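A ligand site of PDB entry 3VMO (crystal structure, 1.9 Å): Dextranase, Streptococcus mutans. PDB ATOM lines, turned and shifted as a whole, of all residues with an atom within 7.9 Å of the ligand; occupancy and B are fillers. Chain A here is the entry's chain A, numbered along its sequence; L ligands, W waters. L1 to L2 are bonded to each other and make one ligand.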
ATOM      1  N   GLN A  38       1.233  -5.935   4.346  1.00  0.00           N
ATOM      2  CA  GLN A  38      -0.063  -6.392   3.942  1.00  0.00           C
ATOM      3  C   GLN A  38      -0.129  -6.471   2.423  1.00  0.00           C
ATOM      4  O   GLN A  38       0.774  -5.990   1.732  1.00  0.00           O
ATOM      5  CB  GLN A  38      -1.143  -5.424   4.414  1.00  0.00           C
ATOM      6  CG  GLN A  38      -0.970  -3.974   3.910  1.00  0.00           C
ATOM      7  CD  GLN A  38      -2.016  -3.055   4.459  1.00  0.00           C
ATOM      8  OE1 GLN A  38      -3.211  -3.340   4.375  1.00  0.00           O
ATOM      9  NE2 GLN A  38      -1.588  -1.967   5.029  1.00  0.00           N
ATOM     10  N   ASN A  39      -1.191  -7.113   1.923  1.00  0.00           N
ATOM     11  CA  ASN A  39      -1.512  -7.075   0.493  1.00  0.00           C
ATOM     12  C   ASN A  39      -1.938  -5.705   0.052  1.00  0.00           C
ATOM     13  O   ASN A  39      -2.773  -5.047   0.696  1.00  0.00           O
ATOM     14  CB  ASN A  39      -2.565  -8.111   0.167  1.00  0.00           C
ATOM     15  CG  ASN A  39      -1.965  -9.532   0.125  1.00  0.00           C
ATOM     16  OD1 ASN A  39      -0.947  -9.779  -0.539  1.00  0.00           O
ATOM     17  ND2 ASN A  39      -2.570 -10.453   0.825  1.00  0.00           N
ATOM     18  N   ILE A  40      -1.327  -5.266  -1.027  1.00  0.00           N
ATOM     19  CA  ILE A  40      -1.645  -3.987  -1.652  1.00  0.00           C
ATOM     20  C   ILE A  40      -2.203  -4.327  -3.041  1.00  0.00           C
ATOM     21  O   ILE A  40      -1.626  -5.160  -3.779  1.00  0.00           O
ATOM     22  CB  ILE A  40      -0.415  -3.075  -1.755  1.00  0.00           C
ATOM     23  CG1 ILE A  40       0.152  -2.719  -0.350  1.00  0.00           C
ATOM     24  CG2 ILE A  40      -0.786  -1.743  -2.461  1.00  0.00           C
ATOM     25  CD1 ILE A  40      -0.772  -1.938   0.509  1.00  0.00           C
ATOM     26  N   THR A  41      -3.357  -3.749  -3.369  1.00  0.00           N
ATOM     27  CA  THR A  41      -4.063  -4.066  -4.620  1.00  0.00           C
ATOM     28  C   THR A  41      -4.115  -2.813  -5.549  1.00  0.00           C
ATOM     29  O   THR A  41      -4.546  -1.719  -5.138  1.00  0.00           O
ATOM     30  CB  THR A  41      -5.493  -4.525  -4.336  1.00  0.00           C
ATOM     31  OG1 THR A  41      -5.485  -5.768  -3.588  1.00  0.00           O
ATOM     32  CG2 THR A  41      -6.293  -4.732  -5.672  1.00  0.00           C
ATOM     33  N   GLN A  57      -6.804  -5.928 -12.392  1.00  0.00           N
ATOM     34  CA  GLN A  57      -6.272  -5.809 -11.012  1.00  0.00           C
ATOM     35  C   GLN A  57      -5.033  -6.593 -10.786  1.00  0.00           C
ATOM     36  O   GLN A  57      -4.774  -7.577 -11.495  1.00  0.00           O
ATOM     37  CB  GLN A  57      -7.319  -6.200 -10.003  1.00  0.00           C
ATOM     38  CG  GLN A  57      -7.327  -7.690  -9.667  1.00  0.00           C
ATOM     39  CD  GLN A  57      -7.109  -7.914  -8.170  1.00  0.00           C
ATOM     40  OE1 GLN A  57      -5.982  -8.221  -7.682  1.00  0.00           O
ATOM     41  NE2 GLN A  57      -8.205  -7.745  -7.426  1.00  0.00           N
ATOM     42  N   TYR A  58      -4.266  -6.220  -9.761  1.00  0.00           N
ATOM     43  CA  TYR A  58      -3.061  -6.936  -9.440  1.00  0.00           C
ATOM     44  C   TYR A  58      -2.757  -6.721  -7.934  1.00  0.00           C
ATOM     45  O   TYR A  58      -2.924  -5.615  -7.443  1.00  0.00           O
ATOM     46  CB  TYR A  58      -1.939  -6.365 -10.262  1.00  0.00           C
ATOM     47  CG  TYR A  58      -0.659  -7.073  -9.980  1.00  0.00           C
ATOM     48  CD1 TYR A  58      -0.301  -8.212 -10.694  1.00  0.00           C
ATOM     49  CD2 TYR A  58       0.190  -6.615  -8.971  1.00  0.00           C
ATOM     50  CE1 TYR A  58       0.882  -8.876 -10.413  1.00  0.00           C
ATOM     51  CE2 TYR A  58       1.380  -7.283  -8.678  1.00  0.00           C
ATOM     52  CZ  TYR A  58       1.723  -8.407  -9.404  1.00  0.00           C
ATOM     53  OH  TYR A  58       2.898  -9.060  -9.124  1.00  0.00           O
ATOM     54  N   THR A  59      -2.393  -7.787  -7.221  1.00  0.00           N
ATOM     55  CA  THR A  59      -2.257  -7.720  -5.736  1.00  0.00           C
ATOM     56  C   THR A  59      -0.925  -8.316  -5.379  1.00  0.00           C
ATOM     57  O   THR A  59      -0.552  -9.387  -5.867  1.00  0.00           O
ATOM     58  CB  THR A  59      -3.383  -8.467  -5.016  1.00  0.00           C
ATOM     59  OG1 THR A  59      -4.629  -7.838  -5.279  1.00  0.00           O
ATOM     60  CG2 THR A  59      -3.198  -8.511  -3.470  1.00  0.00           C
ATOM     61  N   LYS A  60      -0.166  -7.585  -4.554  1.00  0.00           N
ATOM     62  CA  LYS A  60       1.075  -8.106  -4.044  1.00  0.00           C
ATOM     63  C   LYS A  60       1.230  -7.798  -2.547  1.00  0.00           C
ATOM     64  O   LYS A  60       0.946  -6.709  -2.104  1.00  0.00           O
ATOM     65  CB  LYS A  60       2.261  -7.564  -4.810  1.00  0.00           C
ATOM     66  CG  LYS A  60       3.525  -8.416  -4.566  1.00  0.00           C
ATOM     67  CD  LYS A  60       4.638  -7.989  -5.486  1.00  0.00           C
ATOM     68  CE  LYS A  60       6.003  -8.403  -4.975  1.00  0.00           C
ATOM     69  NZ  LYS A  60       6.061  -9.899  -4.811  1.00  0.00           N
ATOM     70  N   TYR A  61       1.715  -8.792  -1.808  1.00  0.00           N
ATOM     71  CA  TYR A  61       2.078  -8.627  -0.398  1.00  0.00           C
ATOM     72  C   TYR A  61       3.380  -7.851  -0.270  1.00  0.00           C
ATOM     73  O   TYR A  61       4.402  -8.219  -0.835  1.00  0.00           O
ATOM     74  CB  TYR A  61       2.133 -10.006   0.280  1.00  0.00           C
ATOM     75  CG  TYR A  61       2.419  -9.971   1.773  1.00  0.00           C
ATOM     76  CD1 TYR A  61       3.735  -9.993   2.257  1.00  0.00           C
ATOM     77  CD2 TYR A  61       1.378  -9.944   2.691  1.00  0.00           C
ATOM     78  CE1 TYR A  61       3.993  -9.967   3.656  1.00  0.00           C
ATOM     79  CE2 TYR A  61       1.627  -9.925   4.076  1.00  0.00           C
ATOM     80  CZ  TYR A  61       2.931  -9.931   4.537  1.00  0.00           C
ATOM     81  OH  TYR A  61       3.164  -9.924   5.895  1.00  0.00           O
ATOM     82  N   LEU A  62       3.327  -6.752   0.454  1.00  0.00           N
ATOM     83  CA  LEU A  62       4.417  -5.815   0.576  1.00  0.00           C
ATOM     84  C   LEU A  62       4.644  -5.482   2.056  1.00  0.00           C
ATOM     85  O   LEU A  62       3.690  -5.271   2.807  1.00  0.00           O
ATOM     86  CB  LEU A  62       4.106  -4.512  -0.179  1.00  0.00           C
ATOM     87  CG  LEU A  62       4.057  -4.631  -1.710  1.00  0.00           C
ATOM     88  CD1 LEU A  62       3.583  -3.309  -2.353  1.00  0.00           C
ATOM     89  CD2 LEU A  62       5.451  -5.018  -2.262  1.00  0.00           C
ATOM     90  N   SER A  95      -5.211   0.241  -3.217  1.00  0.00           N
ATOM     91  CA  SER A  95      -5.903   0.114  -1.945  1.00  0.00           C
ATOM     92  C   SER A  95      -5.130  -0.827  -1.028  1.00  0.00           C
ATOM     93  O   SER A  95      -4.372  -1.652  -1.500  1.00  0.00           O
ATOM     94  CB  SER A  95      -7.357  -0.356  -2.124  1.00  0.00           C
ATOM     95  OG  SER A  95      -7.446  -1.527  -2.912  1.00  0.00           O
ATOM     96  N   ASP A  96      -5.334  -0.694   0.282  1.00  0.00           N
ATOM     97  CA  ASP A  96      -4.709  -1.619   1.211  1.00  0.00           C
ATOM     98  C   ASP A  96      -5.608  -2.843   1.439  1.00  0.00           C
ATOM     99  O   ASP A  96      -6.705  -3.003   0.803  1.00  0.00           O
ATOM    100  CB  ASP A  96      -4.381  -0.890   2.540  1.00  0.00           C
ATOM    101  CG  ASP A  96      -5.618  -0.395   3.282  1.00  0.00           C
ATOM    102  OD1 ASP A  96      -6.755  -0.874   3.049  1.00  0.00           O
ATOM    103  OD2 ASP A  96      -5.480   0.500   4.137  1.00  0.00           O
ATOM    104  N   SER A  97      -5.232  -3.701   2.399  1.00  0.00           N
ATOM    105  CA  SER A  97      -5.997  -4.901   2.576  1.00  0.00           C
ATOM    106  C   SER A  97      -7.348  -4.631   3.281  1.00  0.00           C
ATOM    107  O   SER A  97      -8.215  -5.502   3.309  1.00  0.00           O
ATOM    108  CB  SER A  97      -5.157  -5.972   3.271  1.00  0.00           C
ATOM    109  OG  SER A  97      -4.907  -5.595   4.617  1.00  0.00           O
ATOM    110  N   GLN A  98      -7.540  -3.426   3.811  1.00  0.00           N
ATOM    111  CA  GLN A  98      -8.859  -3.064   4.340  1.00  0.00           C
ATOM    112  C   GLN A  98      -9.698  -2.239   3.321  1.00  0.00           C
ATOM    113  O   GLN A  98     -10.732  -1.646   3.686  1.00  0.00           O
ATOM    114  CB  GLN A  98      -8.763  -2.344   5.704  1.00  0.00           C
ATOM    115  CG  GLN A  98      -8.128  -3.196   6.837  1.00  0.00           C
ATOM    116  CD  GLN A  98      -9.005  -4.376   7.247  1.00  0.00           C
ATOM    117  OE1 GLN A  98      -8.678  -5.554   6.971  1.00  0.00           O
ATOM    118  NE2 GLN A  98     -10.123  -4.087   7.919  1.00  0.00           N
ATOM    119  N   ASN A  99      -9.267  -2.213   2.051  1.00  0.00           N
ATOM    120  CA  ASN A  99      -9.920  -1.413   0.989  1.00  0.00           C
ATOM    121  C   ASN A  99      -9.874   0.099   1.153  1.00  0.00           C
ATOM    122  O   ASN A  99     -10.636   0.801   0.508  1.00  0.00           O
ATOM    123  CB  ASN A  99     -11.378  -1.863   0.759  1.00  0.00           C
ATOM    124  CG  ASN A  99     -11.484  -3.327   0.385  1.00  0.00           C
ATOM    125  OD1 ASN A  99     -10.692  -3.840  -0.398  1.00  0.00           O
ATOM    126  ND2 ASN A  99     -12.471  -4.008   0.945  1.00  0.00           N
HETATM  127  C1  LIG L   1      -2.229 -12.636  -4.792  1.00  0.00           C
HETATM  128  C2  LIG L   1      -1.119 -12.115  -3.853  1.00  0.00           C
HETATM  129  C3  LIG L   1      -1.204 -12.765  -2.450  1.00  0.00           C
HETATM  130  C4  LIG L   1      -2.615 -12.626  -1.878  1.00  0.00           C
HETATM  131  C5  LIG L   1      -3.649 -13.130  -2.897  1.00  0.00           C
HETATM  132  C6  LIG L   1      -5.104 -12.908  -2.462  1.00  0.00           C
HETATM  133  O1  LIG L   1      -2.017 -13.983  -5.181  1.00  0.00           O
HETATM  134  O2  LIG L   1       0.158 -12.268  -4.478  1.00  0.00           O
HETATM  135  O3  LIG L   1      -0.304 -12.147  -1.559  1.00  0.00           O
HETATM  136  O4  LIG L   1      -2.720 -13.264  -0.627  1.00  0.00           O
HETATM  137  O5  LIG L   1      -3.469 -12.454  -4.131  1.00  0.00           O
HETATM  138  O6  LIG L   1      -5.330 -11.519  -2.230  1.00  0.00           O
HETATM  139  C1  LG2 L   2      -6.556 -11.323  -1.488  1.00  0.00           C
HETATM  140  C2  LG2 L   2      -6.821  -9.823  -1.271  1.00  0.00           C
HETATM  141  C3  LG2 L   2      -5.948  -9.235  -0.150  1.00  0.00           C
HETATM  142  C4  LG2 L   2      -6.013 -10.070   1.136  1.00  0.00           C
HETATM  143  C5  LG2 L   2      -5.830 -11.555   0.844  1.00  0.00           C
HETATM  144  C6  LG2 L   2      -6.117 -12.368   2.109  1.00  0.00           C
HETATM  145  O1  LG2 L   2      -6.579  -9.099  -2.469  1.00  0.00           O
HETATM  146  O2  LG2 L   2      -6.265  -7.865   0.137  1.00  0.00           O
HETATM  147  O3  LG2 L   2      -5.003  -9.633   2.042  1.00  0.00           O
HETATM  148  O4  LG2 L   2      -6.616 -12.035  -0.256  1.00  0.00           O
HETATM  149  O5  LG2 L   2      -5.967 -13.740   1.782  1.00  0.00           O
HETATM  150  O   HOH W   1      -8.433  -7.476   1.609  1.00  0.00           O
HETATM  151  O   HOH W   2       2.339 -11.296  -3.277  1.00  0.00           O
HETATM  152  O   HOH W   3      -5.106  -5.743  -0.929  1.00  0.00           O
HETATM  153  O   HOH W   4      -2.963  -8.509   3.984  1.00  0.00           O
HETATM  154  O   HOH W   5      -8.074  -6.469  -2.790  1.00  0.00           O
HETATM  155  O   HOH W   6      -4.498 -15.536   3.059  1.00  0.00           O
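O3 of LIG L1 lies within hydrogen-bond range of OD1 of Asn 39 (2.7 Å). O of Thr 59 lies within hydrogen-bond range of O2 of LIG L1.
OG1 of Thr 59 is in hydrogen-bond range of OE1 of Gln 57. The side-chain hydroxyl (OG) of Ser 97 is in hydrogen-bond range of the side-chain amide oxygen (OE1) of Gln 38. O of Asn 39 lies within hydrogen-bond range of N of Ser 97 (3.3 Å). The side-chain amide oxygen (OD1) of Asn 39 sits at hydrogen-bond distance from the backbone NH (N) of Tyr 61 (3.1 Å). The backbone carbonyl oxygen (O) of Thr 41 is in hydrogen-bond range of the backbone NH (N) of Ser 95. The side-chain hydroxyl of Thr 59 is in hydrogen-bond range of the side-chain hydroxyl of Thr 41, 2.8 Å away.
Thr 41 touches the ligand. CB of Tyr 61 touches O3 of LIG L1, 3.7 Å away. CB of Ser 97 touches O2 of LG2 L2, at 3.8 Å. Hydrophobic or aromatic side chains that line the ligand: Tyr 61. Along chain A the residues within 4 Å of the ligand span positions 39 to 97. The nearest printed residue that does not touch the ligand is Lys 60 (4.3 Å).
Water W3 lies within hydrogen-bond range of an oxygen (O2) of LG2 L2 (2.6 Å), the side-chain hydroxyl (OG1) of Thr 41 (2.7 Å) and the backbone carbonyl oxygen (O) of Asn 39 (2.9 Å). Water W1 lies within hydrogen-bond range of O of Ser 97 (2.6 Å) and O2 of LG2 L2 (2.6 Å). Water W2 bridges O2 of LIG L1 and N of Tyr 61. Water W4 lies within hydrogen-bond range of O3 of LG2 L2 (3.0 Å) and N of Asn 39 (3.1 Å). Water W5 lies within hydrogen-bond range of the side-chain hydroxyl of Thr 41 and an oxygen (O1) of LG2 L2.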
